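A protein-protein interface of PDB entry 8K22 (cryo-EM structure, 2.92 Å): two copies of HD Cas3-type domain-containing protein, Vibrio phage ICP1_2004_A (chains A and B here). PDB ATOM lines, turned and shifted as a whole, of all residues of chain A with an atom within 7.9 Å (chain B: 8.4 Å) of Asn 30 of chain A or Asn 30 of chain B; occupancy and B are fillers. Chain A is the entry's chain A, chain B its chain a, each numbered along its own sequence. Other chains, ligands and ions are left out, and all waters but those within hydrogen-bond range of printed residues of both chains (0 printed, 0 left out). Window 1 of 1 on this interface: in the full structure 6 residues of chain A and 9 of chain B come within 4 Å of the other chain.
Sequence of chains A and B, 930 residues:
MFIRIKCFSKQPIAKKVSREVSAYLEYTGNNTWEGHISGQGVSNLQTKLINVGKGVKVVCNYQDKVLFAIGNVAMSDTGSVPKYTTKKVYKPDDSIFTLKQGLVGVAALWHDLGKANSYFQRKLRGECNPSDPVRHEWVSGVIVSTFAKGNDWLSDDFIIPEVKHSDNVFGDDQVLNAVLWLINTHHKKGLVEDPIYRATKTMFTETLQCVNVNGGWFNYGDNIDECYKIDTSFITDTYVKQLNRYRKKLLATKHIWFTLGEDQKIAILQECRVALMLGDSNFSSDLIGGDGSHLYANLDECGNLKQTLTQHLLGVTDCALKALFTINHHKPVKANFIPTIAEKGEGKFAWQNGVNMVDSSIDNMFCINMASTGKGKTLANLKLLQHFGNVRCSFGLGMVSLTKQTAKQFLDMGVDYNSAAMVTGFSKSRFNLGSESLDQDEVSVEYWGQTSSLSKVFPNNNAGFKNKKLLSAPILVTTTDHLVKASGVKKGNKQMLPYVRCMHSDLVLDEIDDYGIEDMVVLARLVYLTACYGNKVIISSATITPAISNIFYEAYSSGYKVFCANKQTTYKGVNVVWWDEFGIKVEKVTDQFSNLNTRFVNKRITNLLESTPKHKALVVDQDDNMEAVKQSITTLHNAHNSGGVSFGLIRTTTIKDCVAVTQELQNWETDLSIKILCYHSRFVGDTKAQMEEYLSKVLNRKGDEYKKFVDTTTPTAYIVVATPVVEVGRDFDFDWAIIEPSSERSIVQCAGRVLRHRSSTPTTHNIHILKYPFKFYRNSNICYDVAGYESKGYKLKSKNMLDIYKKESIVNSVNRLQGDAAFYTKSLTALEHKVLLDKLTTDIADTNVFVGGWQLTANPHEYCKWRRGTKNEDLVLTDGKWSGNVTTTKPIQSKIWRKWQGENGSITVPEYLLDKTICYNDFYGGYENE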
ATOM      1  N   ILE A   5       5.153  11.946  26.984  1.00  0.00           N
ATOM      2  CA  ILE A   5       4.138  11.255  27.773  1.00  0.00           C
ATOM      3  C   ILE A   5       3.979   9.830  27.263  1.00  0.00           C
ATOM      4  O   ILE A   5       3.712   9.606  26.075  1.00  0.00           O
ATOM      5  CB  ILE A   5       2.799  12.009  27.728  1.00  0.00           C
ATOM      6  CG1 ILE A   5       2.940  13.352  28.446  1.00  0.00           C
ATOM      7  CG2 ILE A   5       1.683  11.162  28.325  1.00  0.00           C
ATOM      8  CD1 ILE A   5       1.639  14.056  28.723  1.00  0.00           C
ATOM      9  N   LYS A   6       4.130   8.866  28.165  1.00  0.00           N
ATOM     10  CA  LYS A   6       3.935   7.456  27.872  1.00  0.00           C
ATOM     11  C   LYS A   6       2.728   6.923  28.635  1.00  0.00           C
ATOM     12  O   LYS A   6       2.425   7.353  29.755  1.00  0.00           O
ATOM     13  CB  LYS A   6       5.186   6.647  28.227  1.00  0.00           C
ATOM     14  CG  LYS A   6       6.258   6.697  27.155  1.00  0.00           C
ATOM     15  CD  LYS A   6       7.644   6.538  27.745  1.00  0.00           C
ATOM     16  CE  LYS A   6       8.276   7.884  28.049  1.00  0.00           C
ATOM     17  NZ  LYS A   6       9.655   7.733  28.589  1.00  0.00           N
ATOM     18  N   CYS A   7       2.035   5.978  28.003  1.00  0.00           N
ATOM     19  CA  CYS A   7       0.799   5.417  28.528  1.00  0.00           C
ATOM     20  C   CYS A   7       0.988   3.943  28.853  1.00  0.00           C
ATOM     21  O   CYS A   7       1.539   3.184  28.051  1.00  0.00           O
ATOM     22  CB  CYS A   7      -0.353   5.590  27.534  1.00  0.00           C
ATOM     23  SG  CYS A   7      -1.126   7.221  27.572  1.00  0.00           S
ATOM     24  N   PHE A   8       0.527   3.549  30.042  1.00  0.00           N
ATOM     25  CA  PHE A   8       0.604   2.163  30.485  1.00  0.00           C
ATOM     26  C   PHE A   8      -0.771   1.515  30.504  1.00  0.00           C
ATOM     27  O   PHE A   8      -0.902   0.383  30.987  1.00  0.00           O
ATOM     28  CB  PHE A   8       1.212   2.039  31.896  1.00  0.00           C
ATOM     29  CG  PHE A   8       2.683   2.364  31.989  1.00  0.00           C
ATOM     30  CD1 PHE A   8       3.163   3.644  31.743  1.00  0.00           C
ATOM     31  CD2 PHE A   8       3.583   1.382  32.373  1.00  0.00           C
ATOM     32  CE1 PHE A   8       4.504   3.927  31.842  1.00  0.00           C
ATOM     33  CE2 PHE A   8       4.928   1.664  32.481  1.00  0.00           C
ATOM     34  CZ  PHE A   8       5.383   2.943  32.222  1.00  0.00           C
ATOM     35  N   SER A   9      -1.790   2.193  29.999  1.00  0.00           N
ATOM     36  CA  SER A   9      -3.155   1.879  30.354  1.00  0.00           C
ATOM     37  C   SER A   9      -3.702   0.719  29.542  1.00  0.00           C
ATOM     38  O   SER A   9      -3.378   0.539  28.366  1.00  0.00           O
ATOM     39  CB  SER A   9      -4.018   3.116  30.161  1.00  0.00           C
ATOM     40  OG  SER A   9      -3.551   3.850  29.047  1.00  0.00           O
ATOM     41  N   TYR A  27       2.012  12.548  18.051  1.00  0.00           N
ATOM     42  CA  TYR A  27       2.035  11.108  18.286  1.00  0.00           C
ATOM     43  C   TYR A  27       3.294  10.524  17.658  1.00  0.00           C
ATOM     44  O   TYR A  27       3.480  10.594  16.438  1.00  0.00           O
ATOM     45  CB  TYR A  27       0.780  10.454  17.712  1.00  0.00           C
ATOM     46  CG  TYR A  27       0.596   9.002  18.093  1.00  0.00           C
ATOM     47  CD1 TYR A  27       0.945   8.544  19.358  1.00  0.00           C
ATOM     48  CD2 TYR A  27       0.058   8.091  17.190  1.00  0.00           C
ATOM     49  CE1 TYR A  27       0.772   7.216  19.712  1.00  0.00           C
ATOM     50  CE2 TYR A  27      -0.120   6.761  17.534  1.00  0.00           C
ATOM     51  CZ  TYR A  27       0.239   6.331  18.796  1.00  0.00           C
ATOM     52  OH  TYR A  27       0.067   5.011  19.143  1.00  0.00           O
ATOM     53  N   THR A  28       4.162   9.948  18.490  1.00  0.00           N
ATOM     54  CA  THR A  28       5.367   9.281  18.020  1.00  0.00           C
ATOM     55  C   THR A  28       5.160   7.784  17.815  1.00  0.00           C
ATOM     56  O   THR A  28       6.119   7.072  17.492  1.00  0.00           O
ATOM     57  CB  THR A  28       6.524   9.523  18.993  1.00  0.00           C
ATOM     58  OG1 THR A  28       6.106   9.205  20.326  1.00  0.00           O
ATOM     59  CG2 THR A  28       6.966  10.977  18.938  1.00  0.00           C
ATOM     60  N   GLY A  29       3.941   7.296  17.997  1.00  0.00           N
ATOM     61  CA  GLY A  29       3.635   5.898  17.798  1.00  0.00           C
ATOM     62  C   GLY A  29       3.830   5.069  19.055  1.00  0.00           C
ATOM     63  O   GLY A  29       4.493   5.474  20.011  1.00  0.00           O
ATOM     64  N   ASN A  30       3.221   3.875  19.029  1.00  0.00           N
ATOM     65  CA  ASN A  30       3.292   2.862  20.092  1.00  0.00           C
ATOM     66  C   ASN A  30       2.818   3.394  21.444  1.00  0.00           C
ATOM     67  O   ASN A  30       3.424   3.093  22.477  1.00  0.00           O
ATOM     68  CB  ASN A  30       4.703   2.273  20.211  1.00  0.00           C
ATOM     69  CG  ASN A  30       4.965   1.171  19.201  1.00  0.00           C
ATOM     70  OD1 ASN A  30       4.083   0.368  18.895  1.00  0.00           O
ATOM     71  ND2 ASN A  30       6.188   1.122  18.685  1.00  0.00           N
ATOM     72  N   ASN A  31       1.728   4.179  21.421  1.00  0.00           N
ATOM     73  CA  ASN A  31       1.126   4.822  22.600  1.00  0.00           C
ATOM     74  C   ASN A  31       2.136   5.683  23.359  1.00  0.00           C
ATOM     75  O   ASN A  31       2.190   5.673  24.590  1.00  0.00           O
ATOM     76  CB  ASN A  31       0.465   3.800  23.532  1.00  0.00           C
ATOM     77  CG  ASN A  31      -0.908   3.363  23.046  1.00  0.00           C
ATOM     78  OD1 ASN A  31      -1.431   3.889  22.061  1.00  0.00           O
ATOM     79  ND2 ASN A  31      -1.502   2.404  23.743  1.00  0.00           N
ATOM     80  N   THR A  32       2.947   6.428  22.613  1.00  0.00           N
ATOM     81  CA  THR A  32       3.916   7.364  23.166  1.00  0.00           C
ATOM     82  C   THR A  32       3.794   8.690  22.431  1.00  0.00           C
ATOM     83  O   THR A  32       3.850   8.723  21.197  1.00  0.00           O
ATOM     84  CB  THR A  32       5.342   6.820  23.041  1.00  0.00           C
ATOM     85  OG1 THR A  32       5.447   5.573  23.738  1.00  0.00           O
ATOM     86  CG2 THR A  32       6.353   7.809  23.603  1.00  0.00           C
ATOM     87  N   TRP A  33       3.632   9.776  23.180  1.00  0.00           N
ATOM     88  CA  TRP A  33       3.565  11.115  22.618  1.00  0.00           C
ATOM     89  C   TRP A  33       4.776  11.900  23.096  1.00  0.00           C
ATOM     90  O   TRP A  33       5.324  11.605  24.160  1.00  0.00           O
ATOM     91  CB  TRP A  33       2.277  11.843  23.014  1.00  0.00           C
ATOM     92  CG  TRP A  33       1.018  11.307  22.388  1.00  0.00           C
ATOM     93  CD1 TRP A  33       0.249  11.940  21.457  1.00  0.00           C
ATOM     94  CD2 TRP A  33       0.316  10.097  22.724  1.00  0.00           C
ATOM     95  NE1 TRP A  33      -0.844  11.176  21.140  1.00  0.00           N
ATOM     96  CE2 TRP A  33      -0.833  10.044  21.909  1.00  0.00           C
ATOM     97  CE3 TRP A  33       0.556   9.047  23.616  1.00  0.00           C
ATOM     98  CZ2 TRP A  33      -1.735   8.984  21.959  1.00  0.00           C
ATOM     99  CZ3 TRP A  33      -0.339   7.995  23.660  1.00  0.00           C
ATOM    100  CH2 TRP A  33      -1.469   7.971  22.837  1.00  0.00           C
ATOM    101  N   LYS A  57      -3.223   5.892  33.163  1.00  0.00           N
ATOM    102  CA  LYS A  57      -1.891   5.384  33.469  1.00  0.00           C
ATOM    103  C   LYS A  57      -0.911   6.192  32.627  1.00  0.00           C
ATOM    104  O   LYS A  57      -0.525   5.767  31.539  1.00  0.00           O
ATOM    105  CB  LYS A  57      -1.798   3.855  33.133  1.00  0.00           C
ATOM    106  CG  LYS A  57      -2.480   2.788  34.056  1.00  0.00           C
ATOM    107  CD  LYS A  57      -2.523   2.884  35.597  1.00  0.00           C
ATOM    108  CE  LYS A  57      -1.289   3.379  36.321  1.00  0.00           C
ATOM    109  NZ  LYS A  57      -1.645   3.542  37.739  1.00  0.00           N
ATOM    110  N   SER A  80      13.072   3.716  33.623  1.00  0.00           N
ATOM    111  CA  SER A  80      11.636   3.929  33.523  1.00  0.00           C
ATOM    112  C   SER A  80      11.006   2.856  32.660  1.00  0.00           C
ATOM    113  O   SER A  80      11.711   2.264  31.842  1.00  0.00           O
ATOM    114  CB  SER A  80      11.326   5.319  32.968  1.00  0.00           C
ATOM    115  OG  SER A  80      10.033   5.745  33.362  1.00  0.00           O
ATOM    116  N   VAL A  81       9.708   2.599  32.840  1.00  0.00           N
ATOM    117  CA  VAL A  81       8.988   1.565  32.089  1.00  0.00           C
ATOM    118  C   VAL A  81       9.509   0.165  32.328  1.00  0.00           C
ATOM    119  O   VAL A  81      10.411  -0.312  31.649  1.00  0.00           O
ATOM    120  CB  VAL A  81       8.845   1.853  30.574  1.00  0.00           C
ATOM    121  CG1 VAL A  81       7.802   0.933  29.956  1.00  0.00           C
ATOM    122  CG2 VAL A  81       8.468   3.308  30.326  1.00  0.00           C
ATOM    123  N   PRO A  82       8.919  -0.520  33.291  1.00  0.00           N
ATOM    124  CA  PRO A  82       9.313  -1.894  33.558  1.00  0.00           C
ATOM    125  C   PRO A  82       8.737  -2.904  32.619  1.00  0.00           C
ATOM    126  O   PRO A  82       8.056  -2.563  31.661  1.00  0.00           O
ATOM    127  CB  PRO A  82       8.622  -2.152  34.859  1.00  0.00           C
ATOM    128  CG  PRO A  82       7.383  -1.351  34.780  1.00  0.00           C
ATOM    129  CD  PRO A  82       7.877  -0.062  34.218  1.00  0.00           C
ATOM    130  N   ARG B   4      16.712   4.993  17.065  1.00  0.00           N
ATOM    131  CA  ARG B   4      15.470   4.637  17.746  1.00  0.00           C
ATOM    132  C   ARG B   4      14.762   3.550  16.951  1.00  0.00           C
ATOM    133  O   ARG B   4      14.493   3.731  15.760  1.00  0.00           O
ATOM    134  CB  ARG B   4      14.567   5.861  17.908  1.00  0.00           C
ATOM    135  CG  ARG B   4      13.210   5.557  18.523  1.00  0.00           C
ATOM    136  CD  ARG B   4      12.436   6.831  18.836  1.00  0.00           C
ATOM    137  NE  ARG B   4      12.174   7.630  17.646  1.00  0.00           N
ATOM    138  CZ  ARG B   4      12.641   8.856  17.449  1.00  0.00           C
ATOM    139  NH1 ARG B   4      13.401   9.459  18.349  1.00  0.00           N
ATOM    140  NH2 ARG B   4      12.336   9.494  16.323  1.00  0.00           N
ATOM    141  N   ILE B   5      14.456   2.436  17.610  1.00  0.00           N
ATOM    142  CA  ILE B   5      13.729   1.319  17.017  1.00  0.00           C
ATOM    143  C   ILE B   5      12.288   1.361  17.504  1.00  0.00           C
ATOM    144  O   ILE B   5      12.037   1.456  18.711  1.00  0.00           O
ATOM    145  CB  ILE B   5      14.387  -0.025  17.377  1.00  0.00           C
ATOM    146  CG1 ILE B   5      15.797  -0.116  16.799  1.00  0.00           C
ATOM    147  CG2 ILE B   5      13.552  -1.197  16.883  1.00  0.00           C
ATOM    148  CD1 ILE B   5      15.856   0.143  15.324  1.00  0.00           C
ATOM    149  N   LYS B   6      11.339   1.300  16.574  1.00  0.00           N
ATOM    150  CA  LYS B   6       9.929   1.154  16.911  1.00  0.00           C
ATOM    151  C   LYS B   6       9.431  -0.189  16.397  1.00  0.00           C
ATOM    152  O   LYS B   6       9.666  -0.543  15.235  1.00  0.00           O
ATOM    153  CB  LYS B   6       9.087   2.294  16.334  1.00  0.00           C
ATOM    154  CG  LYS B   6       9.495   3.677  16.811  1.00  0.00           C
ATOM    155  CD  LYS B   6       8.891   4.759  15.930  1.00  0.00           C
ATOM    156  CE  LYS B   6       9.324   6.146  16.375  1.00  0.00           C
ATOM    157  NZ  LYS B   6       8.784   7.208  15.483  1.00  0.00           N
ATOM    158  N   CYS B   7       8.757  -0.929  17.272  1.00  0.00           N
ATOM    159  CA  CYS B   7       8.205  -2.242  16.968  1.00  0.00           C
ATOM    160  C   CYS B   7       6.688  -2.175  17.046  1.00  0.00           C
ATOM    161  O   CYS B   7       6.138  -1.628  18.008  1.00  0.00           O
ATOM    162  CB  CYS B   7       8.726  -3.297  17.945  1.00  0.00           C
ATOM    163  SG  CYS B   7      10.318  -4.011  17.527  1.00  0.00           S
ATOM    164  N   PHE B   8       6.015  -2.731  16.042  1.00  0.00           N
ATOM    165  CA  PHE B   8       4.560  -2.709  15.953  1.00  0.00           C
ATOM    166  C   PHE B   8       4.008  -4.113  15.720  1.00  0.00           C
ATOM    167  O   PHE B   8       2.957  -4.291  15.102  1.00  0.00           O
ATOM    168  CB  PHE B   8       4.097  -1.775  14.835  1.00  0.00           C
ATOM    169  CG  PHE B   8       4.132  -0.314  15.191  1.00  0.00           C
ATOM    170  CD1 PHE B   8       5.335   0.376  15.234  1.00  0.00           C
ATOM    171  CD2 PHE B   8       2.960   0.371  15.467  1.00  0.00           C
ATOM    172  CE1 PHE B   8       5.371   1.722  15.550  1.00  0.00           C
ATOM    173  CE2 PHE B   8       2.987   1.717  15.787  1.00  0.00           C
ATOM    174  CZ  PHE B   8       4.194   2.392  15.829  1.00  0.00           C
ATOM    175  N   SER B   9       4.698  -5.127  16.230  1.00  0.00           N
ATOM    176  CA  SER B   9       4.451  -6.518  15.877  1.00  0.00           C
ATOM    177  C   SER B   9       3.345  -7.116  16.746  1.00  0.00           C
ATOM    178  O   SER B   9       2.634  -6.422  17.475  1.00  0.00           O
ATOM    179  CB  SER B   9       5.746  -7.322  15.991  1.00  0.00           C
ATOM    180  OG  SER B   9       5.490  -8.685  16.260  1.00  0.00           O
ATOM    181  N   TYR B  27      15.557   0.283  26.826  1.00  0.00           N
ATOM    182  CA  TYR B  27      14.109   0.172  26.676  1.00  0.00           C
ATOM    183  C   TYR B  27      13.477   1.476  27.145  1.00  0.00           C
ATOM    184  O   TYR B  27      13.161   1.653  28.322  1.00  0.00           O
ATOM    185  CB  TYR B  27      13.575  -1.026  27.451  1.00  0.00           C
ATOM    186  CG  TYR B  27      12.119  -1.335  27.182  1.00  0.00           C
ATOM    187  CD1 TYR B  27      11.618  -1.329  25.886  1.00  0.00           C
ATOM    188  CD2 TYR B  27      11.252  -1.654  28.220  1.00  0.00           C
ATOM    189  CE1 TYR B  27      10.287  -1.618  25.632  1.00  0.00           C
ATOM    190  CE2 TYR B  27       9.920  -1.946  27.976  1.00  0.00           C
ATOM    191  CZ  TYR B  27       9.444  -1.925  26.680  1.00  0.00           C
ATOM    192  OH  TYR B  27       8.123  -2.214  26.433  1.00  0.00           O
ATOM    193  N   THR B  28      13.306   2.411  26.205  1.00  0.00           N
ATOM    194  CA  THR B  28      12.567   3.632  26.502  1.00  0.00           C
ATOM    195  C   THR B  28      11.089   3.356  26.730  1.00  0.00           C
ATOM    196  O   THR B  28      10.439   4.101  27.471  1.00  0.00           O
ATOM    197  CB  THR B  28      12.744   4.654  25.379  1.00  0.00           C
ATOM    198  OG1 THR B  28      12.663   3.995  24.109  1.00  0.00           O
ATOM    199  CG2 THR B  28      14.088   5.352  25.512  1.00  0.00           C
ATOM    200  N   GLY B  29      10.546   2.310  26.113  1.00  0.00           N
ATOM    201  CA  GLY B  29       9.279   1.779  26.562  1.00  0.00           C
ATOM    202  C   GLY B  29       8.157   1.658  25.556  1.00  0.00           C
ATOM    203  O   GLY B  29       8.174   2.313  24.509  1.00  0.00           O
ATOM    204  N   ASN B  30       7.169   0.823  25.912  1.00  0.00           N
ATOM    205  CA  ASN B  30       5.986   0.519  25.100  1.00  0.00           C
ATOM    206  C   ASN B  30       6.377   0.002  23.715  1.00  0.00           C
ATOM    207  O   ASN B  30       5.912   0.503  22.689  1.00  0.00           O
ATOM    208  CB  ASN B  30       5.052   1.729  25.001  1.00  0.00           C
ATOM    209  CG  ASN B  30       4.004   1.747  26.096  1.00  0.00           C
ATOM    210  OD1 ASN B  30       3.107   0.905  26.127  1.00  0.00           O
ATOM    211  ND2 ASN B  30       4.114   2.710  27.005  1.00  0.00           N
ATOM    212  N   ASN B  31       7.249  -1.018  23.716  1.00  0.00           N
ATOM    213  CA  ASN B  31       7.812  -1.646  22.512  1.00  0.00           C
ATOM    214  C   ASN B  31       8.517  -0.626  21.616  1.00  0.00           C
ATOM    215  O   ASN B  31       8.399  -0.660  20.389  1.00  0.00           O
ATOM    216  CB  ASN B  31       6.749  -2.430  21.732  1.00  0.00           C
ATOM    217  CG  ASN B  31       6.064  -3.490  22.584  1.00  0.00           C
ATOM    218  OD1 ASN B  31       5.500  -3.191  23.637  1.00  0.00           O
ATOM    219  ND2 ASN B  31       6.110  -4.736  22.125  1.00  0.00           N
ATOM    220  N   THR B  32       9.256   0.291  22.239  1.00  0.00           N
ATOM    221  CA  THR B  32      10.047   1.286  21.523  1.00  0.00           C
ATOM    222  C   THR B  32      11.364   1.470  22.262  1.00  0.00           C
ATOM    223  O   THR B  32      11.367   1.764  23.461  1.00  0.00           O
ATOM    224  CB  THR B  32       9.300   2.621  21.410  1.00  0.00           C
ATOM    225  OG1 THR B  32       8.094   2.432  20.658  1.00  0.00           O
ATOM    226  CG2 THR B  32      10.162   3.666  20.718  1.00  0.00           C
ATOM    227  N   TRP B  33      12.471   1.297  21.548  1.00  0.00           N
ATOM    228  CA  TRP B  33      13.812   1.379  22.108  1.00  0.00           C
ATOM    229  C   TRP B  33      14.519   2.592  21.524  1.00  0.00           C
ATOM    230  O   TRP B  33      14.215   3.006  20.404  1.00  0.00           O
ATOM    231  CB  TRP B  33      14.612   0.113  21.797  1.00  0.00           C
ATOM    232  CG  TRP B  33      14.166  -1.096  22.552  1.00  0.00           C
ATOM    233  CD1 TRP B  33      14.746  -1.627  23.666  1.00  0.00           C
ATOM    234  CD2 TRP B  33      13.046  -1.931  22.245  1.00  0.00           C
ATOM    235  NE1 TRP B  33      14.053  -2.740  24.074  1.00  0.00           N
ATOM    236  CE2 TRP B  33      13.006  -2.948  23.215  1.00  0.00           C
ATOM    237  CE3 TRP B  33      12.074  -1.917  21.240  1.00  0.00           C
ATOM    238  CZ2 TRP B  33      12.029  -3.940  23.214  1.00  0.00           C
ATOM    239  CZ3 TRP B  33      11.108  -2.899  21.241  1.00  0.00           C
ATOM    240  CH2 TRP B  33      11.090  -3.895  22.221  1.00  0.00           C
ATOM    241  N   LYS B  57       8.579  -6.733  12.600  1.00  0.00           N
ATOM    242  CA  LYS B  57       8.046  -5.390  12.425  1.00  0.00           C
ATOM    243  C   LYS B  57       8.963  -4.406  13.139  1.00  0.00           C
ATOM    244  O   LYS B  57       8.804  -4.155  14.334  1.00  0.00           O
ATOM    245  CB  LYS B  57       6.616  -5.328  12.985  1.00  0.00           C
ATOM    246  CG  LYS B  57       5.761  -4.123  12.587  1.00  0.00           C
ATOM    247  CD  LYS B  57       6.011  -3.582  11.192  1.00  0.00           C
ATOM    248  CE  LYS B  57       5.450  -4.562  10.153  1.00  0.00           C
ATOM    249  NZ  LYS B  57       5.293  -3.954   8.840  1.00  0.00           N
ATOM    250  N   VAL B  59      11.015  -0.553  12.619  1.00  0.00           N
ATOM    251  CA  VAL B  59      11.399   0.642  11.885  1.00  0.00           C
ATOM    252  C   VAL B  59      12.487   1.359  12.683  1.00  0.00           C
ATOM    253  O   VAL B  59      12.604   1.206  13.899  1.00  0.00           O
ATOM    254  CB  VAL B  59      10.195   1.564  11.578  1.00  0.00           C
ATOM    255  CG1 VAL B  59       9.880   2.503  12.728  1.00  0.00           C
ATOM    256  CG2 VAL B  59      10.425   2.343  10.293  1.00  0.00           C
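The side-chain amino group (NZ) of Lys 6 of chain B is in hydrogen-bond range of the backbone carbonyl oxygen (O) of Thr 28 of chain A (3.3 Å).
The backbone carbonyl oxygen of Cys 7 of chain B is in hydrogen-bond range of the side-chain amide nitrogen of Asn 30 of chain A.
ND2 of Asn 30 of chain B sits at hydrogen-bond distance from O of Cys 7 of chain A, at 2.8 Å.
The backbone carbonyl oxygen (O) of Asn 31 of chain B is in hydrogen-bond range of the side-chain amide nitrogen (ND2) of Asn 30 of chain A.
The side-chain amide nitrogen (ND2) of Asn 30 of chain A is in hydrogen-bond range of the side-chain hydroxyl (OG1) of Thr 32 of chain B (3.0 Å).
O of Lys 6 of chain B sits at hydrogen-bond distance from N of Val 59 of chain B, 2.9 Å away.
N of Cys 7 of chain B sits at hydrogen-bond distance from O of Asn 31 of chain B, at 3.1 Å.
The side-chain sulfur of Cys 7 of chain B sits close to the backbone carbonyl oxygen of Lys 57 of chain B, at 3.5 Å.
OH of Tyr 27 of chain B sits at hydrogen-bond distance from N of Asn 31 of chain B, 3.1 Å away.
OG1 of Thr 28 of chain B lies within hydrogen-bond range of O of Thr 32 of chain B (2.7 Å).
The side-chain hydroxyl of Thr 28 of chain A is in hydrogen-bond range of the backbone carbonyl oxygen of Thr 32 of chain A, at 2.5 Å.
Among the printed residues, merely in contact across the chains: Asn 30 of chain A with Asn 30 of chain B (3.3 Å), Asn 30 of chain A with Phe 8 of chain B (3.3 Å), Val 81 of chain A with Thr 28 of chain B (3.6 Å), Lys 6 of chain A with Thr 28 of chain B (3.7 Å), Val 81 of chain A with Tyr 27 of chain B (3.8 Å), Val 81 of chain A with Gly 29 of chain B (3.8 Å), Ser 80 of chain A with Tyr 27 of chain B (3.9 Å) and Asn 30 of chain A with Lys 6 of chain B (3.9 Å).
Asn 30 of chain A touches just these residues of chain B: Lys 6, Cys 7, Phe 8, Asn 30, Asn 31 and Thr 32.
Asn 30 of chain B touches just these residues of chain A: Cys 7 (2.8 Å) and Asn 30 (3.3 Å).
No residue of chain B comes within 4 Å of Gly 29 of chain A.
Of the printed residues of chain A, Gly 29 of chain B touches Val 81.
Printed residues of chain A within 4 Å of Asn 31 of chain B: Asn 30.
Of the printed residues of chain B, Lys 6 of chain A touches Thr 28.
Pro 82 of chain A touches none of the printed residues of chain B.
The nearest residue of chain B that does not touch Asn 30 of chain A is Gly 29 of chain B (5.2 Å).
The nearest printed residue of chain B that does not touch Ser 80 of chain A is Thr 28 of chain B (4.9 Å).
Of the 15 printed residues of chain B, 9 touch a printed residue of chain A.
Printed residues of chain A that touch a printed residue of chain B: Lys 6, Cys 7, Thr 28, Asn 30, Ser 80 and Val 81.
Hydrophobic or aromatic side chains of chain A that line the printed part of chain B: Val 81.
Among the printed residues, 13 pairs touch across the chains.
Lys 6 of chain A touches Thr 28 of chain B, and with the chains exchanged Thr 28 of chain A touches Lys 6 of chain B.
Asn 30 of chain A touches Lys 6 of chain B, but with the chains exchanged Lys 6 of chain A does not touch Asn 30 of chain B (4.3 Å).
Asn 30 of chain A touches Phe 8 of chain B, but with the chains exchanged Phe 8 of chain A does not touch Asn 30 of chain B (4.8 Å).
Asn 30 of chain A touches its own counterpart, Asn 30 of chain B.
13 positions are printed for both chains.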
